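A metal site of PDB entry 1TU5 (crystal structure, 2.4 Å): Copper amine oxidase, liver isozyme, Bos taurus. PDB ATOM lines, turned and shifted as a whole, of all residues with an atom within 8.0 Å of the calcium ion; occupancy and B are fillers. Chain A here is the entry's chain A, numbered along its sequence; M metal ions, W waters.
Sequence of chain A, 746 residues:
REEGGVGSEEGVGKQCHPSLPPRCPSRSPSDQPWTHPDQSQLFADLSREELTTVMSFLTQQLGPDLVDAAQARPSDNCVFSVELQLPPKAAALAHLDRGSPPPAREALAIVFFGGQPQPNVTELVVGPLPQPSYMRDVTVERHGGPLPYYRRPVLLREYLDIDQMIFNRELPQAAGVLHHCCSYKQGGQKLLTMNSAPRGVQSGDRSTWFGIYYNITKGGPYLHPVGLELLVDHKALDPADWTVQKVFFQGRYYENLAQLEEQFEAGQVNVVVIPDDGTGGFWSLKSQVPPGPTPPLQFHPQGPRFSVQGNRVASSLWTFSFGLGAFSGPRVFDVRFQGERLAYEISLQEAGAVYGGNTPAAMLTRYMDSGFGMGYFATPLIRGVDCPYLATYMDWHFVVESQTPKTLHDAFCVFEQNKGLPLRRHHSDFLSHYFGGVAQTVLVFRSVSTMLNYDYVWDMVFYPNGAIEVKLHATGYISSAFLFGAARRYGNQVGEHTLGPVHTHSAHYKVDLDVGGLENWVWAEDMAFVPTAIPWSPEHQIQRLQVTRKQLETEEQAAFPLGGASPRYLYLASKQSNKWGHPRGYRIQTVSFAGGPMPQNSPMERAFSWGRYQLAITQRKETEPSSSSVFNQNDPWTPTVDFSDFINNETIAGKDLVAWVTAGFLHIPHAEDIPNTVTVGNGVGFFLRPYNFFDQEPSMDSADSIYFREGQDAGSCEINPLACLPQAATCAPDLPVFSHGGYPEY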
ATOM      1  N   LYS A  89      -7.473 -15.420  13.611  1.00  0.00           N
ATOM      2  CA  LYS A  89      -6.614 -16.538  13.230  1.00  0.00           C
ATOM      3  C   LYS A  89      -5.134 -16.335  13.601  1.00  0.00           C
ATOM      4  O   LYS A  89      -4.483 -17.251  14.105  1.00  0.00           O
ATOM      5  CB  LYS A  89      -6.754 -16.795  11.722  1.00  0.00           C
ATOM      6  CG  LYS A  89      -5.963 -17.975  11.206  1.00  0.00           C
ATOM      7  CD  LYS A  89      -6.114 -18.096   9.713  1.00  0.00           C
ATOM      8  CE  LYS A  89      -5.631 -19.423   9.216  1.00  0.00           C
ATOM      9  NZ  LYS A  89      -5.763 -19.519   7.742  1.00  0.00           N
ATOM     10  N   LEU A 342      -3.676 -29.324   7.825  1.00  0.00           N
ATOM     11  CA  LEU A 342      -4.105 -29.255   6.427  1.00  0.00           C
ATOM     12  C   LEU A 342      -5.094 -28.106   6.301  1.00  0.00           C
ATOM     13  O   LEU A 342      -5.199 -27.455   5.249  1.00  0.00           O
ATOM     14  CB  LEU A 342      -4.858 -30.539   5.997  1.00  0.00           C
ATOM     15  CG  LEU A 342      -4.254 -31.927   6.276  1.00  0.00           C
ATOM     16  CD1 LEU A 342      -5.189 -33.000   5.765  1.00  0.00           C
ATOM     17  CD2 LEU A 342      -2.907 -32.054   5.600  1.00  0.00           C
ATOM     18  N   ALA A 343      -5.837 -27.874   7.365  1.00  0.00           N
ATOM     19  CA  ALA A 343      -6.827 -26.815   7.293  1.00  0.00           C
ATOM     20  C   ALA A 343      -7.081 -26.148   8.638  1.00  0.00           C
ATOM     21  O   ALA A 343      -7.218 -26.825   9.668  1.00  0.00           O
ATOM     22  CB  ALA A 343      -8.136 -27.391   6.716  1.00  0.00           C
ATOM     23  N   TYR A 344      -7.152 -24.822   8.629  1.00  0.00           N
ATOM     24  CA  TYR A 344      -7.419 -24.082   9.847  1.00  0.00           C
ATOM     25  C   TYR A 344      -8.884 -24.317  10.213  1.00  0.00           C
ATOM     26  O   TYR A 344      -9.246 -24.512  11.390  1.00  0.00           O
ATOM     27  CB  TYR A 344      -7.159 -22.578   9.649  1.00  0.00           C
ATOM     28  CG  TYR A 344      -7.452 -21.732  10.876  1.00  0.00           C
ATOM     29  CD1 TYR A 344      -6.745 -21.928  12.068  1.00  0.00           C
ATOM     30  CD2 TYR A 344      -8.483 -20.791  10.869  1.00  0.00           C
ATOM     31  CE1 TYR A 344      -7.081 -21.217  13.227  1.00  0.00           C
ATOM     32  CE2 TYR A 344      -8.818 -20.080  12.028  1.00  0.00           C
ATOM     33  CZ  TYR A 344      -8.123 -20.294  13.201  1.00  0.00           C
ATOM     34  OH  TYR A 344      -8.500 -19.628  14.374  1.00  0.00           O
ATOM     35  N   GLU A 345      -9.736 -24.331   9.183  1.00  0.00           N
ATOM     36  CA  GLU A 345     -11.158 -24.527   9.422  1.00  0.00           C
ATOM     37  C   GLU A 345     -11.904 -25.053   8.219  1.00  0.00           C
ATOM     38  O   GLU A 345     -11.595 -24.686   7.092  1.00  0.00           O
ATOM     39  CB  GLU A 345     -11.804 -23.180   9.840  1.00  0.00           C
ATOM     40  CG  GLU A 345     -13.275 -22.981   9.419  1.00  0.00           C
ATOM     41  CD  GLU A 345     -13.784 -21.552   9.654  1.00  0.00           C
ATOM     42  OE1 GLU A 345     -12.945 -20.609   9.705  1.00  0.00           O
ATOM     43  OE2 GLU A 345     -15.006 -21.369   9.761  1.00  0.00           O
ATOM     44  N   VAL A 511     -13.887 -23.733   3.294  1.00  0.00           N
ATOM     45  CA  VAL A 511     -12.788 -24.658   3.427  1.00  0.00           C
ATOM     46  C   VAL A 511     -11.471 -23.887   3.503  1.00  0.00           C
ATOM     47  O   VAL A 511     -10.878 -23.528   2.467  1.00  0.00           O
ATOM     48  CB  VAL A 511     -12.777 -25.621   2.236  1.00  0.00           C
ATOM     49  CG1 VAL A 511     -11.824 -26.756   2.499  1.00  0.00           C
ATOM     50  CG2 VAL A 511     -14.199 -26.135   1.967  1.00  0.00           C
ATOM     51  N   ASP A 512     -11.023 -23.613   4.722  1.00  0.00           N
ATOM     52  CA  ASP A 512      -9.786 -22.870   4.894  1.00  0.00           C
ATOM     53  C   ASP A 512      -8.540 -23.752   4.961  1.00  0.00           C
ATOM     54  O   ASP A 512      -7.960 -23.972   6.028  1.00  0.00           O
ATOM     55  CB  ASP A 512      -9.853 -21.963   6.130  1.00  0.00           C
ATOM     56  CG  ASP A 512      -8.617 -21.096   6.271  1.00  0.00           C
ATOM     57  OD1 ASP A 512      -7.740 -21.187   5.397  1.00  0.00           O
ATOM     58  OD2 ASP A 512      -8.514 -20.333   7.252  1.00  0.00           O
ATOM     59  N   LEU A 513      -8.144 -24.256   3.803  1.00  0.00           N
ATOM     60  CA  LEU A 513      -6.962 -25.099   3.700  1.00  0.00           C
ATOM     61  C   LEU A 513      -5.700 -24.231   3.887  1.00  0.00           C
ATOM     62  O   LEU A 513      -5.621 -23.122   3.365  1.00  0.00           O
ATOM     63  CB  LEU A 513      -6.910 -25.776   2.317  1.00  0.00           C
ATOM     64  CG  LEU A 513      -7.843 -26.940   1.914  1.00  0.00           C
ATOM     65  CD1 LEU A 513      -7.911 -27.035   0.410  1.00  0.00           C
ATOM     66  CD2 LEU A 513      -7.338 -28.253   2.470  1.00  0.00           C
ATOM     67  N   ASP A 514      -4.741 -24.732   4.640  1.00  0.00           N
ATOM     68  CA  ASP A 514      -3.468 -24.030   4.841  1.00  0.00           C
ATOM     69  C   ASP A 514      -2.471 -25.079   4.406  1.00  0.00           C
ATOM     70  O   ASP A 514      -1.872 -25.789   5.235  1.00  0.00           O
ATOM     71  CB  ASP A 514      -3.229 -23.691   6.306  1.00  0.00           C
ATOM     72  CG  ASP A 514      -3.994 -22.497   6.739  1.00  0.00           C
ATOM     73  OD1 ASP A 514      -4.707 -21.931   5.903  1.00  0.00           O
ATOM     74  OD2 ASP A 514      -3.871 -22.105   7.914  1.00  0.00           O
ATOM     75  N   VAL A 515      -2.299 -25.203   3.095  1.00  0.00           N
ATOM     76  CA  VAL A 515      -1.440 -26.233   2.565  1.00  0.00           C
ATOM     77  C   VAL A 515       0.040 -25.940   2.786  1.00  0.00           C
ATOM     78  O   VAL A 515       0.610 -25.021   2.190  1.00  0.00           O
ATOM     79  CB  VAL A 515      -1.747 -26.417   1.078  1.00  0.00           C
ATOM     80  CG1 VAL A 515      -1.098 -27.693   0.558  1.00  0.00           C
ATOM     81  CG2 VAL A 515      -3.223 -26.468   0.889  1.00  0.00           C
ATOM     82  N   GLY A 517       1.284 -24.644   5.227  1.00  0.00           N
ATOM     83  CA  GLY A 517       1.412 -23.336   5.841  1.00  0.00           C
ATOM     84  C   GLY A 517       0.357 -22.427   5.258  1.00  0.00           C
ATOM     85  O   GLY A 517      -0.482 -22.865   4.477  1.00  0.00           O
ATOM     86  N   LEU A 518       0.420 -21.155   5.627  1.00  0.00           N
ATOM     87  CA  LEU A 518      -0.550 -20.142   5.214  1.00  0.00           C
ATOM     88  C   LEU A 518      -0.487 -19.681   3.771  1.00  0.00           C
ATOM     89  O   LEU A 518      -1.524 -19.594   3.120  1.00  0.00           O
ATOM     90  CB  LEU A 518      -0.415 -18.910   6.122  1.00  0.00           C
ATOM     91  CG  LEU A 518      -1.568 -18.528   7.034  1.00  0.00           C
ATOM     92  CD1 LEU A 518      -1.888 -19.685   7.931  1.00  0.00           C
ATOM     93  CD2 LEU A 518      -1.185 -17.327   7.853  1.00  0.00           C
ATOM     94  N   GLU A 519       0.711 -19.369   3.279  1.00  0.00           N
ATOM     95  CA  GLU A 519       0.889 -18.872   1.914  1.00  0.00           C
ATOM     96  C   GLU A 519       0.566 -19.919   0.846  1.00  0.00           C
ATOM     97  O   GLU A 519       1.298 -20.898   0.688  1.00  0.00           O
ATOM     98  CB  GLU A 519       2.319 -18.377   1.705  1.00  0.00           C
ATOM     99  CG  GLU A 519       2.552 -16.892   1.969  1.00  0.00           C
ATOM    100  CD  GLU A 519       3.944 -16.436   1.489  1.00  0.00           C
ATOM    101  OE1 GLU A 519       4.954 -16.878   2.079  1.00  0.00           O
ATOM    102  OE2 GLU A 519       4.020 -15.658   0.494  1.00  0.00           O
ATOM    103  N   ASN A 520      -0.516 -19.703   0.100  1.00  0.00           N
ATOM    104  CA  ASN A 520      -0.900 -20.678  -0.904  1.00  0.00           C
ATOM    105  C   ASN A 520      -1.135 -20.114  -2.285  1.00  0.00           C
ATOM    106  O   ASN A 520      -1.388 -18.917  -2.455  1.00  0.00           O
ATOM    107  CB  ASN A 520      -2.156 -21.430  -0.479  1.00  0.00           C
ATOM    108  CG  ASN A 520      -1.890 -22.469   0.579  1.00  0.00           C
ATOM    109  OD1 ASN A 520      -2.816 -23.018   1.166  1.00  0.00           O
ATOM    110  ND2 ASN A 520      -0.616 -22.749   0.823  1.00  0.00           N
ATOM    111  N   LEU A 572      -4.941 -26.271  -4.009  1.00  0.00           N
ATOM    112  CA  LEU A 572      -4.250 -25.155  -3.358  1.00  0.00           C
ATOM    113  C   LEU A 572      -2.879 -25.748  -3.035  1.00  0.00           C
ATOM    114  O   LEU A 572      -2.767 -26.897  -2.601  1.00  0.00           O
ATOM    115  CB  LEU A 572      -4.966 -24.721  -2.077  1.00  0.00           C
ATOM    116  CG  LEU A 572      -5.959 -23.584  -2.317  1.00  0.00           C
ATOM    117  CD1 LEU A 572      -7.021 -24.029  -3.310  1.00  0.00           C
ATOM    118  CD2 LEU A 572      -6.572 -23.146  -1.007  1.00  0.00           C
ATOM    119  N   THR A 618     -10.827 -17.268  -2.481  1.00  0.00           N
ATOM    120  CA  THR A 618     -10.638 -15.854  -2.197  1.00  0.00           C
ATOM    121  C   THR A 618      -9.552 -15.727  -1.117  1.00  0.00           C
ATOM    122  O   THR A 618      -9.102 -16.730  -0.569  1.00  0.00           O
ATOM    123  CB  THR A 618     -11.926 -15.214  -1.642  1.00  0.00           C
ATOM    124  OG1 THR A 618     -12.240 -15.786  -0.369  1.00  0.00           O
ATOM    125  CG2 THR A 618     -13.094 -15.457  -2.603  1.00  0.00           C
ATOM    126  N   GLN A 619      -9.138 -14.513  -0.811  1.00  0.00           N
ATOM    127  CA  GLN A 619      -8.172 -14.323   0.270  1.00  0.00           C
ATOM    128  C   GLN A 619      -8.946 -14.418   1.602  1.00  0.00           C
ATOM    129  O   GLN A 619     -10.009 -13.836   1.733  1.00  0.00           O
ATOM    130  CB  GLN A 619      -7.519 -12.936   0.171  1.00  0.00           C
ATOM    131  CG  GLN A 619      -6.298 -12.815  -0.741  1.00  0.00           C
ATOM    132  CD  GLN A 619      -5.787 -11.384  -0.807  1.00  0.00           C
ATOM    133  OE1 GLN A 619      -5.827 -10.669   0.189  1.00  0.00           O
ATOM    134  NE2 GLN A 619      -5.314 -10.965  -1.978  1.00  0.00           N
ATOM    135  N   ARG A 620      -8.404 -15.166   2.555  1.00  0.00           N
ATOM    136  CA  ARG A 620      -9.002 -15.328   3.897  1.00  0.00           C
ATOM    137  C   ARG A 620      -8.960 -13.934   4.494  1.00  0.00           C
ATOM    138  O   ARG A 620      -7.922 -13.315   4.521  1.00  0.00           O
ATOM    139  CB  ARG A 620      -8.113 -16.268   4.739  1.00  0.00           C
ATOM    140  CG  ARG A 620      -8.275 -16.241   6.288  1.00  0.00           C
ATOM    141  CD  ARG A 620      -9.497 -17.018   6.716  1.00  0.00           C
ATOM    142  NE  ARG A 620      -9.644 -17.335   8.146  1.00  0.00           N
ATOM    143  CZ  ARG A 620      -9.629 -16.469   9.157  1.00  0.00           C
ATOM    144  NH1 ARG A 620      -9.425 -15.175   8.970  1.00  0.00           N
ATOM    145  NH2 ARG A 620      -9.946 -16.884  10.379  1.00  0.00           N
ATOM    146  N   LYS A 655      -0.996 -16.157  -0.878  1.00  0.00           N
ATOM    147  CA  LYS A 655      -1.757 -15.536   0.219  1.00  0.00           C
ATOM    148  C   LYS A 655      -2.462 -16.598   1.045  1.00  0.00           C
ATOM    149  O   LYS A 655      -2.437 -17.773   0.690  1.00  0.00           O
ATOM    150  CB  LYS A 655      -2.813 -14.563  -0.339  1.00  0.00           C
ATOM    151  CG  LYS A 655      -2.243 -13.339  -1.034  1.00  0.00           C
ATOM    152  CD  LYS A 655      -1.271 -12.608  -0.133  1.00  0.00           C
ATOM    153  CE  LYS A 655      -0.751 -11.340  -0.787  1.00  0.00           C
ATOM    154  NZ  LYS A 655      -1.850 -10.337  -0.834  1.00  0.00           N
ATOM    155  N   ASP A 656      -3.085 -16.200   2.153  1.00  0.00           N
ATOM    156  CA  ASP A 656      -3.859 -17.137   2.955  1.00  0.00           C
ATOM    157  C   ASP A 656      -5.139 -17.278   2.103  1.00  0.00           C
ATOM    158  O   ASP A 656      -5.891 -16.329   1.908  1.00  0.00           O
ATOM    159  CB  ASP A 656      -4.196 -16.572   4.362  1.00  0.00           C
ATOM    160  CG  ASP A 656      -4.948 -17.579   5.249  1.00  0.00           C
ATOM    161  OD1 ASP A 656      -5.261 -18.685   4.766  1.00  0.00           O
ATOM    162  OD2 ASP A 656      -5.230 -17.268   6.437  1.00  0.00           O
ATOM    163  N   LEU A 657      -5.359 -18.478   1.569  1.00  0.00           N
ATOM    164  CA  LEU A 657      -6.510 -18.708   0.703  1.00  0.00           C
ATOM    165  C   LEU A 657      -7.651 -19.451   1.370  1.00  0.00           C
ATOM    166  O   LEU A 657      -7.446 -20.221   2.304  1.00  0.00           O
ATOM    167  CB  LEU A 657      -6.074 -19.491  -0.534  1.00  0.00           C
ATOM    168  CG  LEU A 657      -5.726 -18.698  -1.815  1.00  0.00           C
ATOM    169  CD1 LEU A 657      -5.203 -17.319  -1.476  1.00  0.00           C
ATOM    170  CD2 LEU A 657      -4.726 -19.499  -2.649  1.00  0.00           C
ATOM    171  N   VAL A 658      -8.850 -19.217   0.901  1.00  0.00           N
ATOM    172  CA  VAL A 658      -9.998 -19.923   1.441  1.00  0.00           C
ATOM    173  C   VAL A 658     -10.830 -20.410   0.274  1.00  0.00           C
ATOM    174  O   VAL A 658     -11.122 -19.661  -0.661  1.00  0.00           O
ATOM    175  CB  VAL A 658     -10.879 -19.028   2.349  1.00  0.00           C
ATOM    176  CG1 VAL A 658     -11.981 -19.866   2.943  1.00  0.00           C
ATOM    177  CG2 VAL A 658     -10.056 -18.457   3.472  1.00  0.00           C
ATOM    178  N   ALA A 659     -11.197 -21.671   0.315  1.00  0.00           N
ATOM    179  CA  ALA A 659     -11.990 -22.246  -0.748  1.00  0.00           C
ATOM    180  C   ALA A 659     -13.422 -22.362  -0.237  1.00  0.00           C
ATOM    181  O   ALA A 659     -13.632 -22.781   0.891  1.00  0.00           O
ATOM    182  CB  ALA A 659     -11.430 -23.629  -1.110  1.00  0.00           C
HETATM  183 CA    CA M   1      -5.849 -20.828   4.011  1.00  0.00          CA
HETATM  184  O   HOH W   1      -4.029 -20.885   2.351  1.00  0.00           O
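Lys 89 touches the calcium ion (NZ to CA, 3.95 Å).
Of the 23 residues printed, 6 come within 4 Å of the calcium ion.
The nearest printed residue that does not touch the calcium ion is Leu 518 (4.6 Å).
Water W1 lies within hydrogen-bond range of the side-chain amide oxygen of Asn 520 (2.7 Å), the backbone NH of Leu 657 (2.9 Å) and the backbone carbonyl oxygen of Leu 518 (2.9 Å).
The side-chain carboxylate of Asp 656 lies within salt-bridge range of the side-chain amino group of Lys 89 (2.7 Å).
The backbone NH (N) of Asp 514 sits at hydrogen-bond distance from the backbone carbonyl oxygen (O) of Leu 342, 2.8 Å away.
The backbone NH of Tyr 344 lies within hydrogen-bond range of the backbone carbonyl oxygen of Asp 512 (2.9 Å).
NZ of Lys 89 is in salt-bridge range of OD2 of Asp 512 (2.9 Å).
The backbone carbonyl oxygen (O) of Glu 345 lies within hydrogen-bond range of the backbone NH (N) of Asp 512, 2.7 Å away.
The side-chain carboxylate (OD2) of Asp 512 lies within salt-bridge range of the guanidinium group (NE) of Arg 620, at 3.3 Å.
The backbone carbonyl oxygen (O) of Asp 656 is in hydrogen-bond range of the backbone NH (N) of Arg 620.
The side-chain amino group (NZ) of Lys 89 is in salt-bridge range of the side-chain carboxylate (OD2) of Asp 514 (3.2 Å).
The calcium ion is bound by OD1 of Asp 656 (2.3 Å), OD1 of Asp 512 (2.4 Å), O of Leu 513 (2.4 Å), O of Leu 657 (2.4 Å), water W1 (2.5 Å) and OD1 of Asp 514 (2.5 Å).
The calcium ion has six donor atoms within binding distance.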
